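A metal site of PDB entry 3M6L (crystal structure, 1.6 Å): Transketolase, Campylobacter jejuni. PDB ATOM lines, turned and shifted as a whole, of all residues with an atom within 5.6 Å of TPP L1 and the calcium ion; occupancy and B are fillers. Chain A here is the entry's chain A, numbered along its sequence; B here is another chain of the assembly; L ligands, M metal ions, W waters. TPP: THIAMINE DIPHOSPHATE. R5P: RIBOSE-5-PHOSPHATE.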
ATOM      1  N   GLY A  33       8.683 -15.442  11.498  1.00  0.00           N
ATOM      2  CA  GLY A  33       9.816 -14.502  11.720  1.00  0.00           C
ATOM      3  C   GLY A  33      10.045 -13.470  10.641  1.00  0.00           C
ATOM      4  O   GLY A  33      10.137 -12.275  10.889  1.00  0.00           O
ATOM      5  N   ALA A  34      10.078 -13.938   9.391  1.00  0.00           N
ATOM      6  CA  ALA A  34      10.287 -13.032   8.261  1.00  0.00           C
ATOM      7  C   ALA A  34       9.122 -12.094   8.067  1.00  0.00           C
ATOM      8  O   ALA A  34       9.311 -10.876   7.848  1.00  0.00           O
ATOM      9  CB  ALA A  34      10.588 -13.788   6.963  1.00  0.00           C
ATOM     10  N   HIS A  70       9.126 -18.401   1.983  1.00  0.00           N
ATOM     11  CA  HIS A  70       8.618 -18.774   3.302  1.00  0.00           C
ATOM     12  C   HIS A  70       7.921 -17.628   3.985  1.00  0.00           C
ATOM     13  O   HIS A  70       7.229 -17.887   4.986  1.00  0.00           O
ATOM     14  CB  HIS A  70       9.737 -19.327   4.192  1.00  0.00           C
ATOM     15  CG  HIS A  70      10.887 -18.401   4.310  1.00  0.00           C
ATOM     16  ND1 HIS A  70      11.118 -17.648   5.418  1.00  0.00           N
ATOM     17  CD2 HIS A  70      11.826 -18.056   3.411  1.00  0.00           C
ATOM     18  CE1 HIS A  70      12.163 -16.865   5.204  1.00  0.00           C
ATOM     19  NE2 HIS A  70      12.619 -17.086   3.988  1.00  0.00           N
ATOM     20  N   GLY A 117      10.295 -20.239  -3.189  1.00  0.00           N
ATOM     21  CA  GLY A 117      10.398 -21.418  -2.285  1.00  0.00           C
ATOM     22  C   GLY A 117      11.830 -21.960  -2.301  1.00  0.00           C
ATOM     23  O   GLY A 117      12.454 -21.990  -1.280  1.00  0.00           O
ATOM     24  N   PRO A 118      12.381 -22.213  -3.451  1.00  0.00           N
ATOM     25  CA  PRO A 118      13.782 -22.580  -3.537  1.00  0.00           C
ATOM     26  C   PRO A 118      14.574 -21.303  -3.512  1.00  0.00           C
ATOM     27  O   PRO A 118      14.392 -20.425  -4.357  1.00  0.00           O
ATOM     28  CB  PRO A 118      13.891 -23.293  -4.882  1.00  0.00           C
ATOM     29  CG  PRO A 118      12.463 -23.679  -5.167  1.00  0.00           C
ATOM     30  CD  PRO A 118      11.637 -22.611  -4.671  1.00  0.00           C
ATOM     31  N   LEU A 119      15.460 -21.159  -2.564  1.00  0.00           N
ATOM     32  CA  LEU A 119      16.089 -19.864  -2.341  1.00  0.00           C
ATOM     33  C   LEU A 119      16.996 -19.480  -3.483  1.00  0.00           C
ATOM     34  O   LEU A 119      17.620 -20.336  -4.236  1.00  0.00           O
ATOM     35  CB  LEU A 119      16.847 -19.890  -1.044  1.00  0.00           C
ATOM     36  CG  LEU A 119      15.990 -19.917   0.222  1.00  0.00           C
ATOM     37  CD1 LEU A 119      16.902 -20.363   1.407  1.00  0.00           C
ATOM     38  CD2 LEU A 119      15.416 -18.526   0.510  1.00  0.00           C
ATOM     39  N   GLY A 154      16.373 -12.508   1.542  1.00  0.00           N
ATOM     40  CA  GLY A 154      16.994 -12.645   2.828  1.00  0.00           C
ATOM     41  C   GLY A 154      18.412 -13.175   2.668  1.00  0.00           C
ATOM     42  O   GLY A 154      18.957 -13.286   1.601  1.00  0.00           O
ATOM     43  N   ASP A 155      18.966 -13.551   3.812  1.00  0.00           N
ATOM     44  CA  ASP A 155      20.343 -14.174   3.895  1.00  0.00           C
ATOM     45  C   ASP A 155      20.469 -15.360   3.007  1.00  0.00           C
ATOM     46  O   ASP A 155      21.507 -15.552   2.346  1.00  0.00           O
ATOM     47  CB  ASP A 155      20.637 -14.587   5.318  1.00  0.00           C
ATOM     48  CG  ASP A 155      20.698 -13.345   6.241  1.00  0.00           C
ATOM     49  OD1 ASP A 155      21.527 -12.435   6.017  1.00  0.00           O
ATOM     50  OD2 ASP A 155      19.902 -13.220   7.187  1.00  0.00           O
ATOM     51  N   GLY A 156      19.487 -16.199   3.053  1.00  0.00           N
ATOM     52  CA  GLY A 156      19.495 -17.433   2.346  1.00  0.00           C
ATOM     53  C   GLY A 156      19.605 -17.201   0.822  1.00  0.00           C
ATOM     54  O   GLY A 156      20.374 -17.887   0.103  1.00  0.00           O
ATOM     55  N   ASP A 157      18.844 -16.253   0.341  1.00  0.00           N
ATOM     56  CA  ASP A 157      18.901 -15.948  -1.101  1.00  0.00           C
ATOM     57  C   ASP A 157      20.327 -15.501  -1.525  1.00  0.00           C
ATOM     58  O   ASP A 157      20.812 -15.833  -2.606  1.00  0.00           O
ATOM     59  CB  ASP A 157      17.931 -14.857  -1.454  1.00  0.00           C
ATOM     60  CG  ASP A 157      16.497 -15.261  -1.249  1.00  0.00           C
ATOM     61  OD1 ASP A 157      16.010 -16.126  -2.022  1.00  0.00           O
ATOM     62  OD2 ASP A 157      15.842 -14.739  -0.324  1.00  0.00           O
ATOM     63  N   GLU A 160      23.188 -18.133  -1.952  1.00  0.00           N
ATOM     64  CA  GLU A 160      23.083 -19.035  -3.138  1.00  0.00           C
ATOM     65  C   GLU A 160      23.803 -18.471  -4.327  1.00  0.00           C
ATOM     66  O   GLU A 160      23.644 -17.274  -4.657  1.00  0.00           O
ATOM     67  CB  GLU A 160      21.640 -19.323  -3.497  1.00  0.00           C
ATOM     68  CG  GLU A 160      20.940 -20.201  -2.548  1.00  0.00           C
ATOM     69  CD  GLU A 160      21.308 -21.680  -2.716  1.00  0.00           C
ATOM     70  OE1 GLU A 160      22.131 -21.987  -3.604  1.00  0.00           O
ATOM     71  OE2 GLU A 160      20.765 -22.521  -1.904  1.00  0.00           O
ATOM     72  N   ASP A 183      16.645  -8.161   3.509  1.00  0.00           N
ATOM     73  CA  ASP A 183      16.287  -8.266   4.915  1.00  0.00           C
ATOM     74  C   ASP A 183      17.469  -8.856   5.660  1.00  0.00           C
ATOM     75  O   ASP A 183      17.618 -10.076   5.799  1.00  0.00           O
ATOM     76  CB  ASP A 183      15.049  -9.183   5.056  1.00  0.00           C
ATOM     77  CG  ASP A 183      14.493  -9.255   6.464  1.00  0.00           C
ATOM     78  OD1 ASP A 183      14.819  -8.329   7.281  1.00  0.00           O
ATOM     79  OD2 ASP A 183      13.741 -10.251   6.773  1.00  0.00           O
ATOM     80  N   ASN A 185      18.757  -9.646   8.901  1.00  0.00           N
ATOM     81  CA  ASN A 185      18.399  -9.881  10.279  1.00  0.00           C
ATOM     82  C   ASN A 185      19.400 -10.725  11.143  1.00  0.00           C
ATOM     83  O   ASN A 185      19.127 -11.063  12.355  1.00  0.00           O
ATOM     84  CB  ASN A 185      16.962 -10.402  10.366  1.00  0.00           C
ATOM     85  CG  ASN A 185      16.814 -11.800   9.789  1.00  0.00           C
ATOM     86  OD1 ASN A 185      17.811 -12.512   9.568  1.00  0.00           O
ATOM     87  ND2 ASN A 185      15.525 -12.201   9.467  1.00  0.00           N
ATOM     88  N   ASN A 186      20.551 -11.066  10.556  1.00  0.00           N
ATOM     89  CA  ASN A 186      21.614 -11.778  11.209  1.00  0.00           C
ATOM     90  C   ASN A 186      21.248 -13.152  11.692  1.00  0.00           C
ATOM     91  O   ASN A 186      21.987 -13.702  12.451  1.00  0.00           O
ATOM     92  CB  ASN A 186      22.150 -10.957  12.422  1.00  0.00           C
ATOM     93  CG  ASN A 186      23.589 -11.346  12.800  1.00  0.00           C
ATOM     94  OD1 ASN A 186      23.889 -11.472  13.975  1.00  0.00           O
ATOM     95  ND2 ASN A 186      24.451 -11.538  11.806  1.00  0.00           N
ATOM     96  N   ILE A 187      20.127 -13.712  11.212  1.00  0.00           N
ATOM     97  CA  ILE A 187      19.674 -15.038  11.684  1.00  0.00           C
ATOM     98  C   ILE A 187      19.337 -15.971  10.544  1.00  0.00           C
ATOM     99  O   ILE A 187      18.802 -15.533   9.560  1.00  0.00           O
ATOM    100  CB  ILE A 187      18.391 -14.875  12.566  1.00  0.00           C
ATOM    101  CG1 ILE A 187      18.805 -14.176  13.903  1.00  0.00           C
ATOM    102  CG2 ILE A 187      17.620 -16.258  12.717  1.00  0.00           C
ATOM    103  CD1 ILE A 187      19.352 -15.107  14.927  1.00  0.00           C
ATOM    104  N   SER A 188      19.716 -17.248  10.669  1.00  0.00           N
ATOM    105  CA  SER A 188      19.216 -18.296   9.741  1.00  0.00           C
ATOM    106  C   SER A 188      18.846 -19.454  10.538  1.00  0.00           C
ATOM    107  O   SER A 188      18.793 -19.370  11.745  1.00  0.00           O
ATOM    108  CB  SER A 188      20.298 -18.631   8.684  1.00  0.00           C
ATOM    109  OG  SER A 188      21.448 -19.244   9.193  1.00  0.00           O
ATOM    110  N   ILE A 189      18.540 -20.595   9.914  1.00  0.00           N
ATOM    111  CA  ILE A 189      17.993 -21.704  10.658  1.00  0.00           C
ATOM    112  C   ILE A 189      18.999 -22.254  11.709  1.00  0.00           C
ATOM    113  O   ILE A 189      18.607 -22.670  12.796  1.00  0.00           O
ATOM    114  CB  ILE A 189      17.588 -22.829   9.664  1.00  0.00           C
ATOM    115  CG1 ILE A 189      16.423 -22.340   8.796  1.00  0.00           C
ATOM    116  CG2 ILE A 189      17.310 -24.114  10.414  1.00  0.00           C
ATOM    117  CD1 ILE A 189      15.893 -23.402   7.769  1.00  0.00           C
ATOM    118  N   VAL A 193      24.050 -15.676  11.527  1.00  0.00           N
ATOM    119  CA  VAL A 193      24.541 -15.704  10.140  1.00  0.00           C
ATOM    120  C   VAL A 193      26.063 -15.752  10.097  1.00  0.00           C
ATOM    121  O   VAL A 193      26.664 -16.332   9.235  1.00  0.00           O
ATOM    122  CB  VAL A 193      23.963 -14.545   9.357  1.00  0.00           C
ATOM    123  CG1 VAL A 193      24.722 -14.254   8.032  1.00  0.00           C
ATOM    124  CG2 VAL A 193      22.460 -14.859   9.037  1.00  0.00           C
ATOM    125  N   ILE A 245      14.504 -10.270  13.287  1.00  0.00           N
ATOM    126  CA  ILE A 245      13.558 -11.352  12.976  1.00  0.00           C
ATOM    127  C   ILE A 245      12.449 -11.392  14.052  1.00  0.00           C
ATOM    128  O   ILE A 245      12.718 -11.189  15.233  1.00  0.00           O
ATOM    129  CB  ILE A 245      14.279 -12.720  12.753  1.00  0.00           C
ATOM    130  CG1 ILE A 245      13.285 -13.709  12.115  1.00  0.00           C
ATOM    131  CG2 ILE A 245      14.733 -13.283  14.040  1.00  0.00           C
ATOM    132  CD1 ILE A 245      13.974 -15.015  11.644  1.00  0.00           C
ATOM    133  N   HIS A 259      12.070 -18.569  13.020  1.00  0.00           N
ATOM    134  CA  HIS A 259      12.149 -18.697  11.549  1.00  0.00           C
ATOM    135  C   HIS A 259      10.985 -19.490  10.984  1.00  0.00           C
ATOM    136  O   HIS A 259      10.382 -19.076   9.965  1.00  0.00           O
ATOM    137  CB  HIS A 259      13.502 -19.338  11.120  1.00  0.00           C
ATOM    138  CG  HIS A 259      13.466 -19.832   9.721  1.00  0.00           C
ATOM    139  ND1 HIS A 259      13.565 -18.984   8.669  1.00  0.00           N
ATOM    140  CD2 HIS A 259      13.156 -21.044   9.195  1.00  0.00           C
ATOM    141  CE1 HIS A 259      13.390 -19.652   7.524  1.00  0.00           C
ATOM    142  NE2 HIS A 259      13.123 -20.908   7.818  1.00  0.00           N
ATOM    143  N   ALA B 366      23.715 -27.633   4.640  1.00  0.00           N
ATOM    144  CA  ALA B 366      23.531 -26.340   4.060  1.00  0.00           C
ATOM    145  C   ALA B 366      22.446 -25.525   4.777  1.00  0.00           C
ATOM    146  O   ALA B 366      21.297 -25.403   4.317  1.00  0.00           O
ATOM    147  CB  ALA B 366      23.267 -26.414   2.536  1.00  0.00           C
ATOM    148  N   ASP B 367      22.795 -25.063   5.961  1.00  0.00           N
ATOM    149  CA  ASP B 367      21.892 -24.324   6.902  1.00  0.00           C
ATOM    150  C   ASP B 367      20.702 -25.094   7.461  1.00  0.00           C
ATOM    151  O   ASP B 367      19.789 -24.451   7.978  1.00  0.00           O
ATOM    152  CB  ASP B 367      21.475 -22.959   6.328  1.00  0.00           C
ATOM    153  CG  ASP B 367      20.860 -21.990   7.406  1.00  0.00           C
ATOM    154  OD1 ASP B 367      21.481 -21.786   8.508  1.00  0.00           O
ATOM    155  OD2 ASP B 367      19.743 -21.435   7.207  1.00  0.00           O
ATOM    156  N   LEU B 368      20.650 -26.425   7.375  1.00  0.00           N
ATOM    157  CA  LEU B 368      19.485 -27.172   7.767  1.00  0.00           C
ATOM    158  C   LEU B 368      19.811 -28.199   8.835  1.00  0.00           C
ATOM    159  O   LEU B 368      19.066 -29.164   9.059  1.00  0.00           O
ATOM    160  CB  LEU B 368      18.871 -27.903   6.584  1.00  0.00           C
ATOM    161  CG  LEU B 368      18.133 -26.967   5.650  1.00  0.00           C
ATOM    162  CD1 LEU B 368      17.689 -27.615   4.311  1.00  0.00           C
ATOM    163  CD2 LEU B 368      16.873 -26.421   6.370  1.00  0.00           C
ATOM    164  N   ILE B 392      23.851 -21.446   3.079  1.00  0.00           N
ATOM    165  CA  ILE B 392      22.873 -21.833   2.047  1.00  0.00           C
ATOM    166  C   ILE B 392      23.621 -21.952   0.715  1.00  0.00           C
ATOM    167  O   ILE B 392      23.444 -21.108  -0.188  1.00  0.00           O
ATOM    168  CB  ILE B 392      21.661 -20.894   2.022  1.00  0.00           C
ATOM    169  CG1 ILE B 392      20.938 -20.770   3.369  1.00  0.00           C
ATOM    170  CG2 ILE B 392      20.564 -21.526   1.129  1.00  0.00           C
ATOM    171  CD1 ILE B 392      21.588 -19.779   4.427  1.00  0.00           C
ATOM    172  N   GLU B 394      24.368 -25.280  -1.223  1.00  0.00           N
ATOM    173  CA  GLU B 394      24.350 -26.700  -1.469  1.00  0.00           C
ATOM    174  C   GLU B 394      25.452 -27.103  -2.446  1.00  0.00           C
ATOM    175  O   GLU B 394      26.100 -28.146  -2.247  1.00  0.00           O
ATOM    176  CB  GLU B 394      22.992 -27.175  -1.980  1.00  0.00           C
ATOM    177  CG  GLU B 394      21.854 -26.992  -1.024  1.00  0.00           C
ATOM    178  CD  GLU B 394      21.218 -25.621  -1.048  1.00  0.00           C
ATOM    179  OE1 GLU B 394      21.627 -24.823  -1.958  1.00  0.00           O
ATOM    180  OE2 GLU B 394      20.280 -25.406  -0.245  1.00  0.00           O
ATOM    181  N   THR B 416      21.219 -31.907   2.973  1.00  0.00           N
ATOM    182  CA  THR B 416      20.154 -30.974   2.697  1.00  0.00           C
ATOM    183  C   THR B 416      18.830 -31.737   2.571  1.00  0.00           C
ATOM    184  O   THR B 416      18.776 -32.957   2.756  1.00  0.00           O
ATOM    185  CB  THR B 416      20.456 -30.044   1.431  1.00  0.00           C
ATOM    186  OG1 THR B 416      19.448 -29.042   1.301  1.00  0.00           O
ATOM    187  CG2 THR B 416      20.672 -31.023   0.258  1.00  0.00           C
ATOM    188  N   PHE B 417      17.777 -30.975   2.302  1.00  0.00           N
ATOM    189  CA  PHE B 417      16.488 -31.590   1.996  1.00  0.00           C
ATOM    190  C   PHE B 417      16.666 -32.259   0.658  1.00  0.00           C
ATOM    191  O   PHE B 417      17.338 -31.714  -0.252  1.00  0.00           O
ATOM    192  CB  PHE B 417      15.343 -30.569   1.925  1.00  0.00           C
ATOM    193  CG  PHE B 417      14.946 -29.889   3.175  1.00  0.00           C
ATOM    194  CD1 PHE B 417      15.068 -30.527   4.393  1.00  0.00           C
ATOM    195  CD2 PHE B 417      14.399 -28.584   3.138  1.00  0.00           C
ATOM    196  CE1 PHE B 417      14.616 -29.851   5.511  1.00  0.00           C
ATOM    197  CE2 PHE B 417      13.976 -27.981   4.254  1.00  0.00           C
ATOM    198  CZ  PHE B 417      14.091 -28.634   5.417  1.00  0.00           C
ATOM    199  N   PHE B 420      16.376 -30.274  -2.570  1.00  0.00           N
ATOM    200  CA  PHE B 420      17.517 -29.398  -2.917  1.00  0.00           C
ATOM    201  C   PHE B 420      18.815 -30.141  -3.252  1.00  0.00           C
ATOM    202  O   PHE B 420      19.861 -29.553  -3.518  1.00  0.00           O
ATOM    203  CB  PHE B 420      17.680 -28.281  -1.863  1.00  0.00           C
ATOM    204  CG  PHE B 420      16.393 -27.478  -1.597  1.00  0.00           C
ATOM    205  CD1 PHE B 420      15.638 -26.985  -2.617  1.00  0.00           C
ATOM    206  CD2 PHE B 420      15.925 -27.300  -0.330  1.00  0.00           C
ATOM    207  CE1 PHE B 420      14.443 -26.265  -2.388  1.00  0.00           C
ATOM    208  CE2 PHE B 420      14.769 -26.590  -0.098  1.00  0.00           C
ATOM    209  CZ  PHE B 420      14.018 -26.157  -1.120  1.00  0.00           C
ATOM    210  N   TYR B 423      20.257 -28.750  -6.408  1.00  0.00           N
ATOM    211  CA  TYR B 423      21.227 -27.673  -6.373  1.00  0.00           C
ATOM    212  C   TYR B 423      22.681 -28.215  -6.345  1.00  0.00           C
ATOM    213  O   TYR B 423      23.560 -27.477  -6.796  1.00  0.00           O
ATOM    214  CB  TYR B 423      21.003 -26.752  -5.224  1.00  0.00           C
ATOM    215  CG  TYR B 423      19.974 -25.682  -5.352  1.00  0.00           C
ATOM    216  CD1 TYR B 423      18.605 -25.970  -5.475  1.00  0.00           C
ATOM    217  CD2 TYR B 423      20.308 -24.311  -5.356  1.00  0.00           C
ATOM    218  CE1 TYR B 423      17.640 -25.035  -5.531  1.00  0.00           C
ATOM    219  CE2 TYR B 423      19.340 -23.338  -5.414  1.00  0.00           C
ATOM    220  CZ  TYR B 423      18.010 -23.660  -5.570  1.00  0.00           C
ATOM    221  OH  TYR B 423      17.077 -22.662  -5.578  1.00  0.00           O
ATOM    222  N   HIS B 456       8.751 -28.032  -2.234  1.00  0.00           N
ATOM    223  CA  HIS B 456       9.509 -28.754  -1.231  1.00  0.00           C
ATOM    224  C   HIS B 456       9.222 -30.251  -1.198  1.00  0.00           C
ATOM    225  O   HIS B 456       9.711 -30.885  -0.261  1.00  0.00           O
ATOM    226  CB  HIS B 456       9.249 -28.135   0.147  1.00  0.00           C
ATOM    227  CG  HIS B 456       9.882 -26.771   0.283  1.00  0.00           C
ATOM    228  ND1 HIS B 456      10.685 -26.394   1.342  1.00  0.00           N
ATOM    229  CD2 HIS B 456       9.829 -25.731  -0.552  1.00  0.00           C
ATOM    230  CE1 HIS B 456      11.088 -25.135   1.117  1.00  0.00           C
ATOM    231  NE2 HIS B 456      10.561 -24.729  -0.017  1.00  0.00           N
HETATM  232  N1' TPP L   1      17.982 -24.437   0.103  1.00  0.00           N
HETATM  233  C2' TPP L   1      17.194 -23.855  -0.800  1.00  0.00           C
HETATM  234  CM2 TPP L   1      17.746 -23.746  -2.211  1.00  0.00           C
HETATM  235  N3' TPP L   1      15.952 -23.355  -0.613  1.00  0.00           N
HETATM  236  C4' TPP L   1      15.379 -23.509   0.580  1.00  0.00           C
HETATM  237  N4' TPP L   1      14.142 -23.066   0.713  1.00  0.00           N
HETATM  238  C5' TPP L   1      16.187 -24.112   1.687  1.00  0.00           C
HETATM  239  C6' TPP L   1      17.469 -24.562   1.372  1.00  0.00           C
HETATM  240  C7' TPP L   1      15.610 -24.246   3.151  1.00  0.00           C
HETATM  241  N3  TPP L   1      15.524 -22.840   3.803  1.00  0.00           N
HETATM  242  C2  TPP L   1      14.468 -21.944   3.891  1.00  0.00           C
HETATM  243  S1  TPP L   1      14.733 -20.319   4.563  1.00  0.00           S
HETATM  244  C5  TPP L   1      16.371 -20.868   4.890  1.00  0.00           C
HETATM  245  C4  TPP L   1      16.596 -22.221   4.371  1.00  0.00           C
HETATM  246  CM4 TPP L   1      17.956 -22.791   4.463  1.00  0.00           C
HETATM  247  C6  TPP L   1      17.444 -20.049   5.574  1.00  0.00           C
HETATM  248  C7  TPP L   1      17.027 -18.883   6.451  1.00  0.00           C
HETATM  249  O7  TPP L   1      16.985 -17.934   5.464  1.00  0.00           O
HETATM  250  PA  TPP L   1      16.759 -16.424   5.512  1.00  0.00           P
HETATM  251  O1A TPP L   1      16.806 -16.072   4.089  1.00  0.00           O
HETATM  252  O2A TPP L   1      17.865 -15.861   6.382  1.00  0.00           O
HETATM  253  O3A TPP L   1      15.363 -16.289   6.209  1.00  0.00           O
HETATM  254  PB  TPP L   1      14.761 -15.675   7.573  1.00  0.00           P
HETATM  255  O1B TPP L   1      13.444 -15.161   7.186  1.00  0.00           O
HETATM  256  O2B TPP L   1      15.717 -14.694   8.183  1.00  0.00           O
HETATM  257  O3B TPP L   1      14.710 -16.778   8.577  1.00  0.00           O
HETATM  258  C1  R5P L   2      12.090 -24.179   3.882  1.00  0.00           C
HETATM  259  O1  R5P L   2      11.686 -22.966   3.164  1.00  0.00           O
HETATM  260  C2  R5P L   2      11.673 -24.135   5.364  1.00  0.00           C
HETATM  261  O2  R5P L   2      12.551 -23.362   6.198  1.00  0.00           O
HETATM  262  C3  R5P L   2      11.270 -25.467   6.058  1.00  0.00           C
HETATM  263  O3  R5P L   2       9.894 -25.138   6.190  1.00  0.00           O
HETATM  264  C4  R5P L   2      11.603 -25.823   7.538  1.00  0.00           C
HETATM  265  O4  R5P L   2      12.942 -25.391   7.863  1.00  0.00           O
HETATM  266  C5  R5P L   2      11.292 -27.311   7.953  1.00  0.00           C
HETATM  267  O5  R5P L   2      11.012 -27.590   9.382  1.00  0.00           O
HETATM  268  P   R5P L   2      10.902 -29.120   9.988  1.00  0.00           P
HETATM  269  O1P R5P L   2      12.305 -29.611  10.670  1.00  0.00           O
HETATM  270  O2P R5P L   2      10.514 -29.961   8.656  1.00  0.00           O
HETATM  271  O3P R5P L   2       9.790 -29.383  10.955  1.00  0.00           O
HETATM  272 CA    CA M   1      17.918 -14.143   7.901  1.00  0.00          CA
HETATM  273  O   HOH W   1      14.797 -15.536   2.423  1.00  0.00           O
HETATM  274  O   HOH W   2      11.000 -16.655   8.842  1.00  0.00           O
HETATM  275  O   HOH W   3      17.092 -12.642   6.232  1.00  0.00           O
HETATM  276  O   HOH W   4      14.258 -12.699   5.767  1.00  0.00           O
HETATM  277  O   HOH W   5      19.976 -26.523   2.105  1.00  0.00           O
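Water W3 lies within hydrogen-bond range of O of Asp 183 and N of Asp 155.
Water W1 lies within hydrogen-bond range of an oxygen (O1A) of TPP L1 (2.7 Å), the side-chain carboxylate (OD2) of Asp 157 (3.0 Å) and a ring nitrogen (NE2) of His 70 (3.1 Å).
Water W4 lies within hydrogen-bond range of OD2 of Asp 183 and O1B of TPP L1.
Water W5 lies within hydrogen-bond range of OE2 of Glu 394 of chain B (2.6 Å), OG1 of Thr 416 of chain B (2.7 Å) and O of Ala 366 of chain B (2.8 Å).
Water W2 lies within hydrogen-bond range of the backbone carbonyl oxygen (O) of His 259, the backbone NH (N) of Ala 34 and an oxygen (O1B) of TPP L1.
Of the 30 residues printed, 3 come within 4 Å of the calcium ion.
The nearest printed residue that does not touch the calcium ion is Ser 188 (4.5 Å).
The calcium ion is bound by O2B of TPP L1, at 2.3 Å.
O2A of TPP L1 is bound to the calcium ion, 2.3 Å away.
OD2 of Asp 155 is bound to the calcium ion (2.3 Å).
The calcium ion is bound by OD1 of Asn 185.
The calcium ion is bound by O of Ile 187 (2.3 Å).
The calcium ion is bound by water W3.
The side-chain carboxylate of Glu 160 lies close to the side-chain carboxylate of Glu 394 of chain B (2.5 Å).
The side-chain hydroxyl (OH) of Tyr 423 of chain B lies within hydrogen-bond range of the backbone carbonyl oxygen (O) of Leu 119 (2.7 Å).
The backbone NH of Ile 189 sits at hydrogen-bond distance from the side-chain carboxylate of Asp 367 of chain B, at 3.1 Å.
OD1 of Asp 367 of chain B sits at hydrogen-bond distance from OG of Ser 188 (2.6 Å).
N of Glu 160 sits close to O of Ile 392 of chain B.
OD2 of Asp 157 sits at hydrogen-bond distance from N of Gly 154, at 3.0 Å.
N4' of TPP L1 lies close to O1 of R5P L2 (3.5 Å).
The backbone NH of Asp 155 is in hydrogen-bond range of an oxygen (O1A) of TPP L1, at 3.3 Å.
O3B of TPP L1 sits at hydrogen-bond distance from ND1 of His 259, 2.5 Å away.
A nitrogen (N1') of TPP L1 sits at hydrogen-bond distance from the side-chain carboxylate (OE2) of Glu 394 of chain B (2.5 Å).
A nitrogen (N4') of TPP L1 is in hydrogen-bond range of the backbone carbonyl oxygen of Gly 117, 2.8 Å away.
O1A of TPP L1 lies within hydrogen-bond range of N of Gly 156 (2.9 Å).
N of Leu 119 is in hydrogen-bond range of N3' of TPP L1.
A ring nitrogen (NE2) of His 259 lies within hydrogen-bond range of an oxygen (O2) of R5P L2 (3.0 Å).
Ala 34 touches TPP L1.
His 70 touches TPP L1 (CE1 to O1B, 2.9 Å).
Pro 118 touches TPP L1 (CA to N3', 3.7 Å).
Gly 154 touches TPP L1 (C to O1A, 3.6 Å).
Glu 160 touches TPP L1.
Ser 188 touches TPP L1.
Ile 189 touches TPP L1.
CD1 of Ile 245 touches O3B of TPP L1, at 3.6 Å.
Asp 367 of chain B touches TPP L1 (OD2 to C6, 3.1 Å).
Ile 392 of chain B touches TPP L1.
Phe 420 of chain B touches TPP L1 (CE2 to C4', 3.2 Å).
Tyr 423 of chain B touches TPP L1 (CZ to CM2, 3.4 Å).
His 456 of chain B touches TPP L1.
Hydrophobic or aromatic side chains within 4 Å of TPP L1: Ala 34, His 70, Leu 119, Ile 189, Ile 245, His 259, Ile 392 of chain B, Phe 420 of chain B, Tyr 423 of chain B and His 456 of chain B.
Within 4 Å of TPP L1: Ala 34, His 70, Gly 117, Pro 118, Leu 119, Gly 154, Asp 155, Gly 156, Glu 160, Asn 185, Ile 187, Ser 188, Ile 189, Ile 245, His 259, Asp 367 of chain B, Ile 392 of chain B, Glu 394 of chain B, Phe 420 of chain B, Tyr 423 of chain B and His 456 of chain B.
The nearest printed residue that does not touch TPP L1 is Leu 368 of chain B (4.1 Å).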
